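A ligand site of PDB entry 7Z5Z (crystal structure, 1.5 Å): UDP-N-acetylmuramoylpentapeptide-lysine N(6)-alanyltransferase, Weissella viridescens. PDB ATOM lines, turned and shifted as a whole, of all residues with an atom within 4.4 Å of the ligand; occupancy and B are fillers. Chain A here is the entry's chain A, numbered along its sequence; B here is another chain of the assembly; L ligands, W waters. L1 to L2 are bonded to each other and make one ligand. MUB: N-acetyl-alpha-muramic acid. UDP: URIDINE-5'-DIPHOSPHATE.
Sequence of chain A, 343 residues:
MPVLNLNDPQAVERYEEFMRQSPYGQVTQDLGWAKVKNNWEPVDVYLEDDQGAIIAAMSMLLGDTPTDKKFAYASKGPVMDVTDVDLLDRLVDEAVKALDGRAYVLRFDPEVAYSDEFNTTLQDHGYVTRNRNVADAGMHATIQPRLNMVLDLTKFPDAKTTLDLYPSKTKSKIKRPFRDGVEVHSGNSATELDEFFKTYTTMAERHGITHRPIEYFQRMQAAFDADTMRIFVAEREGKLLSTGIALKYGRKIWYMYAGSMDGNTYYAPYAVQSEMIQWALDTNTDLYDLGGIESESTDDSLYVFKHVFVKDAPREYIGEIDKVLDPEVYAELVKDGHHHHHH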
ATOM      1  N   LYS A  37     -21.742 -24.616  20.676  1.00  0.00           N
ATOM      2  CA  LYS A  37     -21.614 -24.633  22.136  1.00  0.00           C
ATOM      3  C   LYS A  37     -22.994 -24.639  22.788  1.00  0.00           C
ATOM      4  O   LYS A  37     -23.360 -23.729  23.527  1.00  0.00           O
ATOM      5  CB  LYS A  37     -20.806 -23.427  22.607  1.00  0.00           C
ATOM      6  CG  LYS A  37     -19.427 -23.317  21.950  1.00  0.00           C
ATOM      7  CD  LYS A  37     -18.438 -24.294  22.555  1.00  0.00           C
ATOM      8  CE  LYS A  37     -17.015 -24.016  22.083  1.00  0.00           C
ATOM      9  NZ  LYS A  37     -16.135 -25.127  22.484  1.00  0.00           N
ATOM     10  N   ASN A  39     -24.315 -26.217  25.134  1.00  0.00           N
ATOM     11  CA  ASN A  39     -24.360 -26.295  26.592  1.00  0.00           C
ATOM     12  C   ASN A  39     -24.035 -24.976  27.285  1.00  0.00           C
ATOM     13  O   ASN A  39     -24.006 -24.945  28.522  1.00  0.00           O
ATOM     14  CB  ASN A  39     -23.432 -27.402  27.119  1.00  0.00           C
ATOM     15  CG  ASN A  39     -22.032 -27.341  26.532  1.00  0.00           C
ATOM     16  OD1 ASN A  39     -21.843 -26.915  25.389  1.00  0.00           O
ATOM     17  ND2 ASN A  39     -21.037 -27.755  27.314  1.00  0.00           N
ATOM     18  N   TRP A  40     -23.821 -23.902  26.525  1.00  0.00           N
ATOM     19  CA  TRP A  40     -23.551 -22.571  27.049  1.00  0.00           C
ATOM     20  C   TRP A  40     -24.719 -21.658  26.705  1.00  0.00           C
ATOM     21  O   TRP A  40     -25.455 -21.906  25.754  1.00  0.00           O
ATOM     22  CB  TRP A  40     -22.269 -22.019  26.400  1.00  0.00           C
ATOM     23  CG  TRP A  40     -21.024 -22.771  26.764  1.00  0.00           C
ATOM     24  CD1 TRP A  40     -20.719 -24.079  26.443  1.00  0.00           C
ATOM     25  CD2 TRP A  40     -19.918 -22.279  27.526  1.00  0.00           C
ATOM     26  NE1 TRP A  40     -19.502 -24.408  26.959  1.00  0.00           N
ATOM     27  CE2 TRP A  40     -18.980 -23.322  27.615  1.00  0.00           C
ATOM     28  CE3 TRP A  40     -19.611 -21.033  28.102  1.00  0.00           C
ATOM     29  CZ2 TRP A  40     -17.760 -23.174  28.284  1.00  0.00           C
ATOM     30  CZ3 TRP A  40     -18.419 -20.888  28.779  1.00  0.00           C
ATOM     31  CH2 TRP A  40     -17.511 -21.953  28.871  1.00  0.00           C
ATOM     32  N   ASP A  64     -21.267 -22.711  33.387  1.00  0.00           N
ATOM     33  CA  ASP A  64     -21.413 -22.922  34.817  1.00  0.00           C
ATOM     34  C   ASP A  64     -20.046 -22.997  35.502  1.00  0.00           C
ATOM     35  O   ASP A  64     -19.013 -23.244  34.868  1.00  0.00           O
ATOM     36  CB  ASP A  64     -22.198 -24.217  35.071  1.00  0.00           C
ATOM     37  CG  ASP A  64     -23.654 -24.106  34.642  1.00  0.00           C
ATOM     38  OD1 ASP A  64     -24.331 -23.152  35.098  1.00  0.00           O
ATOM     39  OD2 ASP A  64     -24.120 -24.971  33.875  1.00  0.00           O
ATOM     40  N   THR A  65     -20.056 -22.781  36.809  1.00  0.00           N
ATOM     41  CA  THR A  65     -18.895 -22.892  37.687  1.00  0.00           C
ATOM     42  C   THR A  65     -19.356 -23.606  38.953  1.00  0.00           C
ATOM     43  O   THR A  65     -20.564 -23.789  39.151  1.00  0.00           O
ATOM     44  CB  THR A  65     -18.380 -21.506  38.079  1.00  0.00           C
ATOM     45  OG1 THR A  65     -19.261 -20.932  39.049  1.00  0.00           O
ATOM     46  CG2 THR A  65     -18.273 -20.581  36.855  1.00  0.00           C
ATOM     47  N   PHE A  71     -19.482 -18.063  34.231  1.00  0.00           N
ATOM     48  CA  PHE A  71     -18.275 -17.634  33.531  1.00  0.00           C
ATOM     49  C   PHE A  71     -18.706 -17.121  32.156  1.00  0.00           C
ATOM     50  O   PHE A  71     -19.273 -17.881  31.357  1.00  0.00           O
ATOM     51  CB  PHE A  71     -17.347 -18.839  33.394  1.00  0.00           C
ATOM     52  CG  PHE A  71     -16.138 -18.614  32.495  1.00  0.00           C
ATOM     53  CD1 PHE A  71     -15.160 -17.705  32.853  1.00  0.00           C
ATOM     54  CD2 PHE A  71     -15.982 -19.329  31.323  1.00  0.00           C
ATOM     55  CE1 PHE A  71     -14.055 -17.491  32.055  1.00  0.00           C
ATOM     56  CE2 PHE A  71     -14.859 -19.121  30.512  1.00  0.00           C
ATOM     57  CZ  PHE A  71     -13.899 -18.206  30.883  1.00  0.00           C
ATOM     58  N   TYR A 104     -19.058 -13.806  37.114  1.00  0.00           N
ATOM     59  CA  TYR A 104     -17.980 -13.289  37.935  1.00  0.00           C
ATOM     60  C   TYR A 104     -16.892 -12.613  37.134  1.00  0.00           C
ATOM     61  O   TYR A 104     -16.122 -11.823  37.682  1.00  0.00           O
ATOM     62  CB  TYR A 104     -17.390 -14.397  38.821  1.00  0.00           C
ATOM     63  CG  TYR A 104     -16.450 -15.368  38.112  1.00  0.00           C
ATOM     64  CD1 TYR A 104     -16.934 -16.522  37.491  1.00  0.00           C
ATOM     65  CD2 TYR A 104     -15.064 -15.162  38.123  1.00  0.00           C
ATOM     66  CE1 TYR A 104     -16.080 -17.419  36.857  1.00  0.00           C
ATOM     67  CE2 TYR A 104     -14.203 -16.068  37.517  1.00  0.00           C
ATOM     68  CZ  TYR A 104     -14.711 -17.186  36.887  1.00  0.00           C
ATOM     69  OH  TYR A 104     -13.836 -18.074  36.284  1.00  0.00           O
ATOM     70  N   ARG A 107     -14.428 -12.717  30.100  1.00  0.00           N
ATOM     71  CA  ARG A 107     -13.112 -12.986  29.534  1.00  0.00           C
ATOM     72  C   ARG A 107     -13.185 -12.907  28.016  1.00  0.00           C
ATOM     73  O   ARG A 107     -14.133 -13.409  27.406  1.00  0.00           O
ATOM     74  CB  ARG A 107     -12.653 -14.396  29.927  1.00  0.00           C
ATOM     75  CG  ARG A 107     -11.371 -14.844  29.195  1.00  0.00           C
ATOM     76  CD  ARG A 107     -10.779 -16.091  29.820  1.00  0.00           C
ATOM     77  NE  ARG A 107     -10.274 -15.805  31.160  1.00  0.00           N
ATOM     78  CZ  ARG A 107      -9.986 -16.717  32.073  1.00  0.00           C
ATOM     79  NH1 ARG A 107     -10.081 -18.008  31.811  1.00  0.00           N
ATOM     80  NH2 ARG A 107      -9.608 -16.312  33.284  1.00  0.00           N
ATOM     81  N   ILE A 143      -7.336 -20.735  27.789  1.00  0.00           N
ATOM     82  CA  ILE A 143      -8.278 -21.639  27.138  1.00  0.00           C
ATOM     83  C   ILE A 143      -7.822 -21.935  25.709  1.00  0.00           C
ATOM     84  O   ILE A 143      -7.697 -23.093  25.304  1.00  0.00           O
ATOM     85  CB  ILE A 143      -9.695 -21.031  27.162  1.00  0.00           C
ATOM     86  CG1 ILE A 143     -10.164 -20.854  28.616  1.00  0.00           C
ATOM     87  CG2 ILE A 143     -10.657 -21.908  26.367  1.00  0.00           C
ATOM     88  CD1 ILE A 143     -11.454 -20.074  28.762  1.00  0.00           C
ATOM     89  N   THR A 210      -8.144 -36.276  25.436  1.00  0.00           N
ATOM     90  CA  THR A 210      -9.592 -36.168  25.391  1.00  0.00           C
ATOM     91  C   THR A 210     -10.056 -35.679  24.006  1.00  0.00           C
ATOM     92  O   THR A 210      -9.289 -35.083  23.236  1.00  0.00           O
ATOM     93  CB  THR A 210     -10.088 -35.239  26.496  1.00  0.00           C
ATOM     94  OG1 THR A 210      -9.523 -33.928  26.334  1.00  0.00           O
ATOM     95  CG2 THR A 210      -9.680 -35.790  27.858  1.00  0.00           C
ATOM     96  N   HIS A 211     -11.321 -35.943  23.714  1.00  0.00           N
ATOM     97  CA  HIS A 211     -11.912 -35.766  22.392  1.00  0.00           C
ATOM     98  C   HIS A 211     -13.409 -35.554  22.492  1.00  0.00           C
ATOM     99  O   HIS A 211     -14.066 -36.077  23.401  1.00  0.00           O
ATOM    100  CB  HIS A 211     -11.557 -36.947  21.478  1.00  0.00           C
ATOM    101  CG  HIS A 211     -12.164 -38.242  21.913  1.00  0.00           C
ATOM    102  ND1 HIS A 211     -13.229 -38.843  21.270  1.00  0.00           N
ATOM    103  CD2 HIS A 211     -11.832 -39.067  22.940  1.00  0.00           C
ATOM    104  CE1 HIS A 211     -13.517 -39.981  21.871  1.00  0.00           C
ATOM    105  NE2 HIS A 211     -12.699 -40.130  22.896  1.00  0.00           N
ATOM    106  N   ARG A 212     -13.957 -34.769  21.527  1.00  0.00           N
ATOM    107  CA  ARG A 212     -15.339 -34.317  21.541  1.00  0.00           C
ATOM    108  C   ARG A 212     -16.251 -35.327  20.862  1.00  0.00           C
ATOM    109  O   ARG A 212     -15.830 -36.065  19.957  1.00  0.00           O
ATOM    110  CB  ARG A 212     -15.445 -32.968  20.824  1.00  0.00           C
ATOM    111  CG  ARG A 212     -14.546 -31.893  21.421  1.00  0.00           C
ATOM    112  CD  ARG A 212     -14.861 -30.571  20.801  1.00  0.00           C
ATOM    113  NE  ARG A 212     -14.065 -29.477  21.341  1.00  0.00           N
ATOM    114  CZ  ARG A 212     -14.439 -28.734  22.373  1.00  0.00           C
ATOM    115  NH1 ARG A 212     -15.559 -28.974  23.021  1.00  0.00           N
ATOM    116  NH2 ARG A 212     -13.675 -27.715  22.756  1.00  0.00           N
ATOM    117  N   PRO A 213     -17.511 -35.403  21.294  1.00  0.00           N
ATOM    118  CA  PRO A 213     -18.450 -36.344  20.688  1.00  0.00           C
ATOM    119  C   PRO A 213     -18.841 -35.918  19.276  1.00  0.00           C
ATOM    120  O   PRO A 213     -18.699 -34.755  18.905  1.00  0.00           O
ATOM    121  CB  PRO A 213     -19.665 -36.313  21.620  1.00  0.00           C
ATOM    122  CG  PRO A 213     -19.502 -35.117  22.482  1.00  0.00           C
ATOM    123  CD  PRO A 213     -18.113 -34.604  22.381  1.00  0.00           C
ATOM    124  N   TYR A 216     -20.920 -32.734  18.431  1.00  0.00           N
ATOM    125  CA  TYR A 216     -20.300 -31.423  18.377  1.00  0.00           C
ATOM    126  C   TYR A 216     -20.056 -31.008  16.942  1.00  0.00           C
ATOM    127  O   TYR A 216     -20.390 -29.895  16.517  1.00  0.00           O
ATOM    128  CB  TYR A 216     -18.960 -31.506  19.108  1.00  0.00           C
ATOM    129  CG  TYR A 216     -18.244 -30.195  19.321  1.00  0.00           C
ATOM    130  CD1 TYR A 216     -18.558 -29.387  20.412  1.00  0.00           C
ATOM    131  CD2 TYR A 216     -17.260 -29.763  18.439  1.00  0.00           C
ATOM    132  CE1 TYR A 216     -17.893 -28.188  20.617  1.00  0.00           C
ATOM    133  CE2 TYR A 216     -16.598 -28.556  18.629  1.00  0.00           C
ATOM    134  CZ  TYR A 216     -16.917 -27.786  19.738  1.00  0.00           C
ATOM    135  OH  TYR A 216     -16.255 -26.597  19.945  1.00  0.00           O
ATOM    136  N   ALA B   1     -10.565 -31.055  26.817  1.00  0.00           N
ATOM    137  CA  ALA B   1      -9.488 -30.489  27.614  1.00  0.00           C
ATOM    138  C   ALA B   1      -8.143 -30.556  26.894  1.00  0.00           C
ATOM    139  O   ALA B   1      -7.273 -29.711  27.111  1.00  0.00           O
ATOM    140  CB  ALA B   1      -9.408 -31.184  28.974  1.00  0.00           C
ATOM    141  N   FGA B   2      -7.970 -31.557  26.036  1.00  0.00           N
ATOM    142  CA  FGA B   2      -6.702 -31.726  25.339  1.00  0.00           C
ATOM    143  C   FGA B   2      -5.907 -32.801  26.009  1.00  0.00           C
ATOM    144  O   FGA B   2      -6.457 -33.711  26.637  1.00  0.00           O
ATOM    145  CB  FGA B   2      -6.948 -32.065  23.867  1.00  0.00           C
ATOM    146  CG  FGA B   2      -7.685 -30.952  23.124  1.00  0.00           C
ATOM    147  CD  FGA B   2      -6.774 -29.798  22.763  1.00  0.00           C
ATOM    148  OE1 FGA B   2      -5.708 -29.603  23.329  1.00  0.00           O
ATOM    149  OXT FGA B   2      -4.573 -32.781  25.928  1.00  0.00           O
ATOM    150  N   CYS B   3      -7.715 -28.970  22.061  1.00  0.00           N
ATOM    151  CA  CYS B   3      -6.881 -27.784  21.872  1.00  0.00           C
ATOM    152  C   CYS B   3      -7.789 -26.559  21.727  1.00  0.00           C
ATOM    153  O   CYS B   3      -7.752 -25.858  20.722  1.00  0.00           O
ATOM    154  CB  CYS B   3      -5.982 -27.981  20.640  1.00  0.00           C
ATOM    155  SG  CYS B   3      -4.726 -26.704  20.386  1.00  0.00           S
ATOM    156  N   DAL B   4      -8.599 -26.319  22.751  1.00  0.00           N
ATOM    157  CA  DAL B   4      -9.615 -25.272  22.701  1.00  0.00           C
ATOM    158  CB  DAL B   4     -10.354 -25.177  24.029  1.00  0.00           C
ATOM    159  C   DAL B   4     -10.596 -25.564  21.570  1.00  0.00           C
ATOM    160  O   DAL B   4     -11.019 -26.715  21.405  1.00  0.00           O
ATOM    161  N   DAL B   5     -10.944 -24.522  20.812  1.00  0.00           N
ATOM    162  CA  DAL B   5     -11.820 -24.679  19.641  1.00  0.00           C
ATOM    163  CB  DAL B   5     -11.988 -23.356  18.923  1.00  0.00           C
ATOM    164  C   DAL B   5     -13.196 -25.243  20.016  1.00  0.00           C
ATOM    165  O   DAL B   5     -13.740 -26.082  19.294  1.00  0.00           O
ATOM    166  OXT DAL B   5     -13.767 -24.876  21.047  1.00  0.00           O
HETATM  167  C1  MUB L   1     -15.682 -28.878  27.384  1.00  0.00           C
HETATM  168  C2  MUB L   1     -14.331 -29.561  27.139  1.00  0.00           C
HETATM  169  C3  MUB L   1     -14.476 -30.643  26.073  1.00  0.00           C
HETATM  170  C4  MUB L   1     -15.661 -31.556  26.383  1.00  0.00           C
HETATM  171  C5  MUB L   1     -16.923 -30.717  26.562  1.00  0.00           C
HETATM  172  C6  MUB L   1     -18.155 -31.522  26.888  1.00  0.00           C
HETATM  173  C7  MUB L   1     -12.348 -28.163  27.496  1.00  0.00           C
HETATM  174  C8  MUB L   1     -11.453 -27.105  26.923  1.00  0.00           C
HETATM  175  C9  MUB L   1     -12.325 -31.045  25.020  1.00  0.00           C
HETATM  176  C10 MUB L   1     -11.049 -30.454  25.611  1.00  0.00           C
HETATM  177  C11 MUB L   1     -12.014 -32.292  24.226  1.00  0.00           C
HETATM  178  O1  MUB L   1     -16.038 -28.301  26.169  1.00  0.00           O
HETATM  179  O3  MUB L   1     -13.262 -31.399  26.032  1.00  0.00           O
HETATM  180  O4  MUB L   1     -15.879 -32.473  25.317  1.00  0.00           O
HETATM  181  O5  MUB L   1     -16.719 -29.812  27.670  1.00  0.00           O
HETATM  182  O6  MUB L   1     -18.011 -32.142  28.158  1.00  0.00           O
HETATM  183  O7  MUB L   1     -12.137 -28.654  28.605  1.00  0.00           O
HETATM  184  O10 MUB L   1     -10.483 -29.516  24.984  1.00  0.00           O
HETATM  185  N2  MUB L   1     -13.368 -28.551  26.739  1.00  0.00           N
HETATM  186  N1  UDP L   2     -13.340 -22.154  32.128  1.00  0.00           N
HETATM  187  C2  UDP L   2     -12.624 -21.162  32.758  1.00  0.00           C
HETATM  188  N3  UDP L   2     -13.243 -20.581  33.823  1.00  0.00           N
HETATM  189  C4  UDP L   2     -14.491 -20.891  34.323  1.00  0.00           C
HETATM  190  C5  UDP L   2     -15.168 -21.943  33.624  1.00  0.00           C
HETATM  191  C6  UDP L   2     -14.589 -22.534  32.565  1.00  0.00           C
HETATM  192  O2  UDP L   2     -11.501 -20.813  32.393  1.00  0.00           O
HETATM  193  O4  UDP L   2     -14.925 -20.284  35.313  1.00  0.00           O
HETATM  194  C1' UDP L   2     -12.701 -22.832  30.995  1.00  0.00           C
HETATM  195  C2' UDP L   2     -12.651 -24.344  31.151  1.00  0.00           C
HETATM  196  O2' UDP L   2     -11.605 -24.705  32.048  1.00  0.00           O
HETATM  197  C3' UDP L   2     -12.390 -24.759  29.701  1.00  0.00           C
HETATM  198  C4' UDP L   2     -13.079 -23.647  28.890  1.00  0.00           C
HETATM  199  O4' UDP L   2     -13.475 -22.638  29.841  1.00  0.00           O
HETATM  200  O3' UDP L   2     -11.005 -24.751  29.396  1.00  0.00           O
HETATM  201  C5' UDP L   2     -14.270 -24.079  28.093  1.00  0.00           C
HETATM  202  O5' UDP L   2     -13.814 -24.961  27.036  1.00  0.00           O
HETATM  203  PA  UDP L   2     -14.694 -25.222  25.775  1.00  0.00           P
HETATM  204  O1A UDP L   2     -14.886 -23.931  25.088  1.00  0.00           O
HETATM  205  O2A UDP L   2     -14.125 -26.382  24.963  1.00  0.00           O
HETATM  206  O3A UDP L   2     -16.093 -25.729  26.377  1.00  0.00           O
HETATM  207  PB  UDP L   2     -16.907 -27.020  25.971  1.00  0.00           P
HETATM  208  O1B UDP L   2     -17.223 -26.820  24.494  1.00  0.00           O
HETATM  209  O3B UDP L   2     -18.187 -26.933  26.810  1.00  0.00           O
HETATM  210  O   HOH W   1     -10.456 -29.234  22.118  1.00  0.00           O
HETATM  211  O   HOH W   2     -18.066 -27.000  29.544  1.00  0.00           O
HETATM  212  O   HOH W   3     -19.737 -27.745  23.769  1.00  0.00           O
HETATM  213  O   HOH W   4      -9.989 -27.302  30.115  1.00  0.00           O
HETATM  214  O   HOH W   5      -8.069 -27.569  25.207  1.00  0.00           O
HETATM  215  O   HOH W   6     -17.294 -31.204  23.088  1.00  0.00           O
HETATM  216  O   HOH W   7     -12.215 -32.821  28.437  1.00  0.00           O
HETATM  217  O   HOH W   8     -15.180 -22.562  37.126  1.00  0.00           O
HETATM  218  O   HOH W   9     -13.294 -23.130  22.978  1.00  0.00           O
HETATM  219  O   HOH W  10     -10.414 -20.439  35.706  1.00  0.00           O
HETATM  220  O   HOH W  11     -16.876 -22.011  25.251  1.00  0.00           O
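Merely in contact with the ligand: Thr 65 (3.7 Å), Phe 71 (3.4 Å), Ile 143 (3.4 Å), Thr 210 (3.7 Å), His 211 (3.8 Å) and DAL 4 of chain B (3.6 Å).
Of the 19 residues printed, 14 come within 4 Å of the ligand.
Along chain A the residues within 4 Å of the ligand span positions 37 to 212.
Water W9 lies within hydrogen-bond range of OXT of DAL 5 of chain B (2.6 Å) and an oxygen (O1A) of UDP L2 (2.8 Å).
Water W3 lies within hydrogen-bond range of O1B of UDP L2 (2.8 Å) and OD1 of Asn 39 (2.8 Å).
Water W1 lies within hydrogen-bond range of O of DAL 4 of chain B (2.7 Å), N of Cys 3 of chain B (2.8 Å) and O10 of MUB L1 (2.9 Å).
Water W6 lies within hydrogen-bond range of NH1 of Arg 212 (2.8 Å) and O4 of MUB L1 (2.9 Å).
Water W7 bridges the backbone NH of Ala 1 of chain B (2.9 Å) and an oxygen (O3) of MUB L1 (3.0 Å).
Water W5 lies within hydrogen-bond range of N of DAL 4 of chain B (2.8 Å), the backbone carbonyl oxygen (O) of Ala 1 of chain B (3.0 Å), an oxygen (O10) of MUB L1 (3.1 Å) and the backbone NH (N) of Cys 3 of chain B (3.5 Å).
OG1 of Thr 210 sits at hydrogen-bond distance from N of Ala 1 of chain B (3.1 Å).
The guanidinium group (NH2) of Arg 212 lies within hydrogen-bond range of O of DAL 4 of chain B, at 3.1 Å.
NH2 of Arg 212 lies within salt-bridge range of OXT of DAL 5 of chain B, 3.3 Å away.
The side-chain amino group (NZ) of Lys 37 lies within hydrogen-bond range of the side-chain hydroxyl (OH) of Tyr 216 (2.9 Å).
NZ of Lys 37 is in salt-bridge range of OXT of DAL 5 of chain B, 2.8 Å away.
N of FGA 2 of chain B is in hydrogen-bond range of the side-chain hydroxyl (OG1) of Thr 210.
N of Ala 1 of chain B is bonded to C10 of MUB L1 (1.4 Å).
O2A of UDP L2 lies within salt-bridge range of NH2 of Arg 212, 2.6 Å away.
OH of Tyr 104 is in hydrogen-bond range of O4 of UDP L2 (2.6 Å).
The side-chain amino group (NZ) of Lys 37 lies within salt-bridge range of an oxygen (O1B) of UDP L2, at 2.8 Å.
The indole nitrogen (NE1) of Trp 40 lies within hydrogen-bond range of an oxygen (O3B) of UDP L2.
The side-chain amide nitrogen (ND2) of Asn 39 sits at hydrogen-bond distance from an oxygen (O3B) of UDP L2 (3.0 Å).
The guanidinium group of Arg 107 sits at hydrogen-bond distance from an oxygen (O2) of UDP L2.
N of FGA 2 of chain B sits close to an oxygen (O10) of MUB L1 (3.4 Å).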
